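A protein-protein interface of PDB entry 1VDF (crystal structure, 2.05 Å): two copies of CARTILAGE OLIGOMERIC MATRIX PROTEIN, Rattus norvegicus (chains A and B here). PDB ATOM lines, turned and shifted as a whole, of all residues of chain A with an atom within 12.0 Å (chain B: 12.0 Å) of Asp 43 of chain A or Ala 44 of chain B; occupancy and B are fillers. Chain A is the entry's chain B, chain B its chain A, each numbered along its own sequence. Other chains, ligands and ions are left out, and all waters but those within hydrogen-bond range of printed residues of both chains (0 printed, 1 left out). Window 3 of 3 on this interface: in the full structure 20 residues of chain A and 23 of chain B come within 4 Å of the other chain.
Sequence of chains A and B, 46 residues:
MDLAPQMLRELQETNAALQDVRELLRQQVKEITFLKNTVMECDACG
Along chain A the printed residues that touch a printed residue of chain B span positions 35 to 44.
Printed residues of chain B that touch a printed residue of chain A: Lys 36, Val 39, Ala 44, Cys 45 and Gly 46.
Among the printed residues, no Asp or Glu carboxylate lies within 4 Å of a Lys or Arg side-chain nitrogen of the other chain.
Thr 38 of chain A touches Val 39 of chain B, but with the chains exchanged Val 39 of chain A does not touch Thr 38 of chain B (8.7 Å).
Asp 43 of chain A touches Ala 44 of chain B, but with the chains exchanged Ala 44 of chain A does not touch Asp 43 of chain B (6.6 Å).
Asp 43 of chain A touches Gly 46 of chain B, but with the chains exchanged Gly 46 of chain A does not touch Asp 43 of chain B (11.6 Å).
Ala 44 of chain A touches its own counterpart, Ala 44 of chain B.
Positions printed for both chains: 36, 37, 38, 39, 40, 41, 42, 43, 44, 45 and 46.
Of the 12 pairs that touch across the chains among the printed residues, 1 has its exchanged pair printed and touching as well.
The side-chain sulfur (SG) of Cys 42 of chain A is disulfide-bonded to the side-chain sulfur (SG) of Cys 45 of chain B (2.0 Å).
N of Ala 44 of chain A sits at hydrogen-bond distance from O of Ala 44 of chain B, 3.0 Å away.
The chain-end carboxylate (OXT) of Gly 46 of chain B sits close to the backbone carbonyl oxygen (O) of Thr 38 of chain A.
The chain-end carboxylate of Gly 46 of chain B sits close to the backbone carbonyl oxygen of Glu 41 of chain A.
Asp 43 of chain A touches three residues of chain B.
Of the printed residues of chain A, Ala 44 of chain B touches Cys 42 (3.9 Å), Asp 43 (3.9 Å) and Ala 44 (3.0 Å).
Printed residues of chain B within 4 Å of Cys 42 of chain A: Ala 44 (3.9 Å), Cys 45 (2.0 Å) and Gly 46 (3.8 Å).
Ala 44 of chain A touches just one residue of chain B: Ala 44.
No residue of chain B comes within 4 Å of Cys 45 of chain A.
Cys 42 of chain B touches none of the printed residues of chain A.
No residue of chain A comes within 4 Å of Asp 43 of chain B.
Cys 45 of chain B touches just these residues of chain A: Cys 42 and Asp 43.
Printed residues of chain B within 4 Å of Thr 38 of chain A: Val 39 and Gly 46.
Of the printed residues of chain B, Leu 35 of chain A touches Lys 36 (3.7 Å) and Val 39 (3.8 Å).
Asn 37 of chain A touches none of the printed residues of chain B.
The nearest residue of chain B that does not touch Asp 43 of chain A is Asp 43 of chain B (6.4 Å).
The nearest printed residue of chain B that does not touch Thr 38 of chain A is Met 40 of chain B (4.2 Å).
Among the printed residues, merely in contact across the chains: Leu 35 of chain A with Lys 36 of chain B, Cys 42 of chain A with Gly 46 of chain B, Asp 43 of chain A with Cys 45 of chain B, Leu 35 of chain A with Val 39 of chain B, Cys 42 of chain A with Ala 44 of chain B, Asp 43 of chain A with Ala 44 of chain B, Asp 43 of chain A with Gly 46 of chain B and Thr 38 of chain A with Val 39 of chain B.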
ATOM      1  N   LEU A  35       7.859 -22.716 -21.371  1.00  0.00           N
ATOM      2  CA  LEU A  35       6.871 -23.266 -20.471  1.00  0.00           C
ATOM      3  C   LEU A  35       5.490 -23.073 -21.129  1.00  0.00           C
ATOM      4  O   LEU A  35       4.710 -24.017 -21.233  1.00  0.00           O
ATOM      5  CB  LEU A  35       6.960 -22.572 -19.104  1.00  0.00           C
ATOM      6  CG  LEU A  35       6.004 -23.070 -18.031  1.00  0.00           C
ATOM      7  CD1 LEU A  35       6.339 -24.507 -17.692  1.00  0.00           C
ATOM      8  CD2 LEU A  35       6.120 -22.191 -16.802  1.00  0.00           C
ATOM      9  N   LYS A  36       5.220 -21.854 -21.619  1.00  0.00           N
ATOM     10  CA  LYS A  36       3.953 -21.532 -22.292  1.00  0.00           C
ATOM     11  C   LYS A  36       3.534 -22.568 -23.336  1.00  0.00           C
ATOM     12  O   LYS A  36       2.412 -23.038 -23.300  1.00  0.00           O
ATOM     13  CB  LYS A  36       3.989 -20.136 -22.931  1.00  0.00           C
ATOM     14  CG  LYS A  36       2.672 -19.723 -23.591  1.00  0.00           C
ATOM     15  CD  LYS A  36       2.825 -18.530 -24.532  1.00  0.00           C
ATOM     16  CE  LYS A  36       3.785 -18.798 -25.700  1.00  0.00           C
ATOM     17  NZ  LYS A  36       3.929 -17.628 -26.613  1.00  0.00           N
ATOM     18  N   ASN A  37       4.421 -22.888 -24.281  1.00  0.00           N
ATOM     19  CA  ASN A  37       4.112 -23.878 -25.325  1.00  0.00           C
ATOM     20  C   ASN A  37       3.885 -25.292 -24.774  1.00  0.00           C
ATOM     21  O   ASN A  37       2.941 -25.970 -25.158  1.00  0.00           O
ATOM     22  CB  ASN A  37       5.199 -23.902 -26.421  1.00  0.00           C
ATOM     23  CG  ASN A  37       5.386 -22.552 -27.075  1.00  0.00           C
ATOM     24  OD1 ASN A  37       4.434 -21.775 -27.223  1.00  0.00           O
ATOM     25  ND2 ASN A  37       6.616 -22.252 -27.450  1.00  0.00           N
ATOM     26  N   THR A  38       4.774 -25.713 -23.880  1.00  0.00           N
ATOM     27  CA  THR A  38       4.708 -27.015 -23.255  1.00  0.00           C
ATOM     28  C   THR A  38       3.363 -27.197 -22.628  1.00  0.00           C
ATOM     29  O   THR A  38       2.747 -28.238 -22.732  1.00  0.00           O
ATOM     30  CB  THR A  38       5.761 -27.144 -22.156  1.00  0.00           C
ATOM     31  OG1 THR A  38       7.064 -27.134 -22.751  1.00  0.00           O
ATOM     32  CG2 THR A  38       5.540 -28.442 -21.356  1.00  0.00           C
ATOM     33  N   VAL A  39       2.908 -26.157 -21.959  1.00  0.00           N
ATOM     34  CA  VAL A  39       1.617 -26.219 -21.334  1.00  0.00           C
ATOM     35  C   VAL A  39       0.569 -26.256 -22.438  1.00  0.00           C
ATOM     36  O   VAL A  39      -0.434 -26.968 -22.335  1.00  0.00           O
ATOM     37  CB  VAL A  39       1.405 -25.070 -20.371  1.00  0.00           C
ATOM     38  CG1 VAL A  39      -0.086 -24.838 -20.150  1.00  0.00           C
ATOM     39  CG2 VAL A  39       2.098 -25.398 -19.039  1.00  0.00           C
ATOM     40  N   MET A  40       0.844 -25.533 -23.533  1.00  0.00           N
ATOM     41  CA  MET A  40      -0.045 -25.490 -24.688  1.00  0.00           C
ATOM     42  C   MET A  40      -0.274 -26.854 -25.331  1.00  0.00           C
ATOM     43  O   MET A  40      -1.298 -27.091 -25.981  1.00  0.00           O
ATOM     44  CB  MET A  40       0.448 -24.491 -25.727  1.00  0.00           C
ATOM     45  CG  MET A  40       0.390 -23.052 -25.232  1.00  0.00           C
ATOM     46  SD  MET A  40      -0.628 -21.948 -26.253  1.00  0.00           S
ATOM     47  CE  MET A  40      -1.878 -23.124 -26.827  1.00  0.00           C
ATOM     48  N   GLU A  41       0.675 -27.753 -25.148  1.00  0.00           N
ATOM     49  CA  GLU A  41       0.575 -29.095 -25.717  1.00  0.00           C
ATOM     50  C   GLU A  41       0.364 -30.161 -24.632  1.00  0.00           C
ATOM     51  O   GLU A  41       0.623 -31.336 -24.846  1.00  0.00           O
ATOM     52  CB  GLU A  41       1.797 -29.440 -26.614  1.00  0.00           C
ATOM     53  CG  GLU A  41       1.409 -29.987 -28.019  1.00  0.00           C
ATOM     54  CD  GLU A  41       2.454 -30.908 -28.653  1.00  0.00           C
ATOM     55  OE1 GLU A  41       3.416 -30.343 -29.280  1.00  0.00           O
ATOM     56  OE2 GLU A  41       2.323 -32.142 -28.608  1.00  0.00           O
ATOM     57  N   CYS A  42      -0.117 -29.743 -23.466  1.00  0.00           N
ATOM     58  CA  CYS A  42      -0.379 -30.674 -22.402  1.00  0.00           C
ATOM     59  C   CYS A  42      -1.690 -31.428 -22.695  1.00  0.00           C
ATOM     60  O   CYS A  42      -2.779 -30.844 -22.674  1.00  0.00           O
ATOM     61  CB  CYS A  42      -0.473 -29.940 -21.067  1.00  0.00           C
ATOM     62  SG  CYS A  42      -0.819 -31.045 -19.675  1.00  0.00           S
ATOM     63  N   ASP A  43      -1.573 -32.725 -22.981  1.00  0.00           N
ATOM     64  CA  ASP A  43      -2.731 -33.540 -23.301  1.00  0.00           C
ATOM     65  C   ASP A  43      -3.898 -33.320 -22.349  1.00  0.00           C
ATOM     66  O   ASP A  43      -5.028 -33.124 -22.794  1.00  0.00           O
ATOM     67  CB  ASP A  43      -2.364 -35.036 -23.360  1.00  0.00           C
ATOM     68  CG  ASP A  43      -3.499 -35.898 -23.887  1.00  0.00           C
ATOM     69  OD1 ASP A  43      -3.955 -35.691 -25.018  1.00  0.00           O
ATOM     70  OD2 ASP A  43      -3.960 -36.815 -23.107  1.00  0.00           O
ATOM     71  N   ALA A  44      -3.615 -33.373 -21.042  1.00  0.00           N
ATOM     72  CA  ALA A  44      -4.623 -33.243 -19.985  1.00  0.00           C
ATOM     73  C   ALA A  44      -5.503 -31.999 -20.011  1.00  0.00           C
ATOM     74  O   ALA A  44      -6.442 -31.888 -19.225  1.00  0.00           O
ATOM     75  CB  ALA A  44      -3.970 -33.388 -18.621  1.00  0.00           C
ATOM     76  N   CYS A  45      -5.216 -31.057 -20.892  1.00  0.00           N
ATOM     77  CA  CYS A  45      -6.009 -29.845 -20.901  1.00  0.00           C
ATOM     78  C   CYS A  45      -7.239 -29.835 -21.789  1.00  0.00           C
ATOM     79  O   CYS A  45      -8.112 -28.994 -21.632  1.00  0.00           O
ATOM     80  CB  CYS A  45      -5.129 -28.600 -21.072  1.00  0.00           C
ATOM     81  SG  CYS A  45      -4.065 -28.328 -19.628  1.00  0.00           S
ATOM     82  N   GLY A  46      -7.311 -30.783 -22.708  1.00  0.00           N
ATOM     83  CA  GLY A  46      -8.463 -30.871 -23.592  1.00  0.00           C
ATOM     84  C   GLY A  46      -8.083 -30.669 -25.050  1.00  0.00           C
ATOM     85  O   GLY A  46      -7.014 -31.186 -25.455  1.00  0.00           O
ATOM     86  OXT GLY A  46      -8.859 -29.987 -25.759  1.00  0.00           O
ATOM     87  N   LYS B  36       9.805 -25.504 -15.242  1.00  0.00           N
ATOM     88  CA  LYS B  36       9.631 -25.916 -16.603  1.00  0.00           C
ATOM     89  C   LYS B  36       9.967 -27.376 -16.735  1.00  0.00           C
ATOM     90  O   LYS B  36       9.199 -28.176 -17.262  1.00  0.00           O
ATOM     91  CB  LYS B  36      10.520 -25.121 -17.530  1.00  0.00           C
ATOM     92  CG  LYS B  36      10.605 -25.778 -18.923  1.00  0.00           C
ATOM     93  CD  LYS B  36      11.806 -25.266 -19.715  1.00  0.00           C
ATOM     94  CE  LYS B  36      13.098 -25.912 -19.296  1.00  0.00           C
ATOM     95  NZ  LYS B  36      14.236 -25.193 -19.877  1.00  0.00           N
ATOM     96  N   ASN B  37      11.141 -27.722 -16.250  1.00  0.00           N
ATOM     97  CA  ASN B  37      11.557 -29.084 -16.352  1.00  0.00           C
ATOM     98  C   ASN B  37      10.542 -29.999 -15.691  1.00  0.00           C
ATOM     99  O   ASN B  37      10.226 -31.084 -16.202  1.00  0.00           O
ATOM    100  CB  ASN B  37      13.000 -29.253 -15.868  1.00  0.00           C
ATOM    101  CG  ASN B  37      14.033 -28.783 -16.933  1.00  0.00           C
ATOM    102  OD1 ASN B  37      14.195 -29.411 -17.988  1.00  0.00           O
ATOM    103  ND2 ASN B  37      14.742 -27.708 -16.635  1.00  0.00           N
ATOM    104  N   THR B  38       9.973 -29.525 -14.597  1.00  0.00           N
ATOM    105  CA  THR B  38       8.956 -30.279 -13.874  1.00  0.00           C
ATOM    106  C   THR B  38       7.729 -30.530 -14.741  1.00  0.00           C
ATOM    107  O   THR B  38       7.222 -31.669 -14.821  1.00  0.00           O
ATOM    108  CB  THR B  38       8.610 -29.557 -12.534  1.00  0.00           C
ATOM    109  OG1 THR B  38       9.812 -29.428 -11.761  1.00  0.00           O
ATOM    110  CG2 THR B  38       7.599 -30.343 -11.731  1.00  0.00           C
ATOM    111  N   VAL B  39       7.279 -29.480 -15.421  1.00  0.00           N
ATOM    112  CA  VAL B  39       6.104 -29.590 -16.280  1.00  0.00           C
ATOM    113  C   VAL B  39       6.349 -30.494 -17.487  1.00  0.00           C
ATOM    114  O   VAL B  39       5.440 -31.182 -17.986  1.00  0.00           O
ATOM    115  CB  VAL B  39       5.584 -28.227 -16.693  1.00  0.00           C
ATOM    116  CG1 VAL B  39       4.360 -28.384 -17.548  1.00  0.00           C
ATOM    117  CG2 VAL B  39       5.225 -27.397 -15.463  1.00  0.00           C
ATOM    118  N   MET B  40       7.594 -30.517 -17.935  1.00  0.00           N
ATOM    119  CA  MET B  40       7.960 -31.348 -19.060  1.00  0.00           C
ATOM    120  C   MET B  40       7.819 -32.821 -18.757  1.00  0.00           C
ATOM    121  O   MET B  40       7.590 -33.635 -19.658  1.00  0.00           O
ATOM    122  CB  MET B  40       9.376 -31.009 -19.500  1.00  0.00           C
ATOM    123  CG  MET B  40       9.396 -29.659 -20.181  1.00  0.00           C
ATOM    124  SD  MET B  40      11.059 -29.284 -20.661  1.00  0.00           S
ATOM    125  CE  MET B  40      11.330 -30.681 -21.785  1.00  0.00           C
ATOM    126  N   GLU B  41       7.951 -33.130 -17.463  1.00  0.00           N
ATOM    127  CA  GLU B  41       7.823 -34.478 -16.919  1.00  0.00           C
ATOM    128  C   GLU B  41       6.468 -34.705 -16.237  1.00  0.00           C
ATOM    129  O   GLU B  41       6.295 -35.656 -15.466  1.00  0.00           O
ATOM    130  CB  GLU B  41       8.976 -34.794 -15.956  1.00  0.00           C
ATOM    131  CG  GLU B  41      10.330 -34.331 -16.488  1.00  0.00           C
ATOM    132  CD  GLU B  41      10.824 -35.290 -17.507  1.00  0.00           C
ATOM    133  OE1 GLU B  41      10.137 -36.293 -17.728  1.00  0.00           O
ATOM    134  OE2 GLU B  41      11.950 -35.035 -18.069  1.00  0.00           O
ATOM    135  N   CYS B  42       5.497 -33.851 -16.544  1.00  0.00           N
ATOM    136  CA  CYS B  42       4.168 -34.036 -16.002  1.00  0.00           C
ATOM    137  C   CYS B  42       3.413 -35.094 -16.831  1.00  0.00           C
ATOM    138  O   CYS B  42       2.892 -34.824 -17.953  1.00  0.00           O
ATOM    139  CB  CYS B  42       3.371 -32.745 -15.955  1.00  0.00           C
ATOM    140  SG  CYS B  42       1.762 -33.052 -15.174  1.00  0.00           S
ATOM    141  N   ASP B  43       3.363 -36.302 -16.267  1.00  0.00           N
ATOM    142  CA  ASP B  43       2.731 -37.420 -16.953  1.00  0.00           C
ATOM    143  C   ASP B  43       1.383 -37.174 -17.601  1.00  0.00           C
ATOM    144  O   ASP B  43       1.102 -37.730 -18.644  1.00  0.00           O
ATOM    145  CB  ASP B  43       2.852 -38.740 -16.169  1.00  0.00           C
ATOM    146  CG  ASP B  43       4.299 -39.052 -15.782  1.00  0.00           C
ATOM    147  OD1 ASP B  43       5.221 -38.301 -16.138  1.00  0.00           O
ATOM    148  OD2 ASP B  43       4.497 -40.103 -15.072  1.00  0.00           O
ATOM    149  N   ALA B  44       0.558 -36.316 -17.013  1.00  0.00           N
ATOM    150  CA  ALA B  44      -0.744 -36.015 -17.612  1.00  0.00           C
ATOM    151  C   ALA B  44      -0.574 -35.131 -18.827  1.00  0.00           C
ATOM    152  O   ALA B  44      -1.536 -34.858 -19.547  1.00  0.00           O
ATOM    153  CB  ALA B  44      -1.686 -35.341 -16.611  1.00  0.00           C
ATOM    154  N   CYS B  45       0.658 -34.667 -19.040  1.00  0.00           N
ATOM    155  CA  CYS B  45       0.935 -33.773 -20.159  1.00  0.00           C
ATOM    156  C   CYS B  45       1.512 -34.357 -21.440  1.00  0.00           C
ATOM    157  O   CYS B  45       1.339 -35.519 -21.791  1.00  0.00           O
ATOM    158  CB  CYS B  45       1.833 -32.597 -19.733  1.00  0.00           C
ATOM    159  SG  CYS B  45       0.983 -31.320 -18.799  1.00  0.00           S
ATOM    160  N   GLY B  46       2.205 -33.450 -22.125  1.00  0.00           N
ATOM    161  CA  GLY B  46       2.871 -33.659 -23.392  1.00  0.00           C
ATOM    162  C   GLY B  46       3.181 -32.282 -23.988  1.00  0.00           C
ATOM    163  O   GLY B  46       3.263 -32.204 -25.240  1.00  0.00           O
ATOM    164  OXT GLY B  46       3.301 -31.292 -23.189  1.00  0.00           O
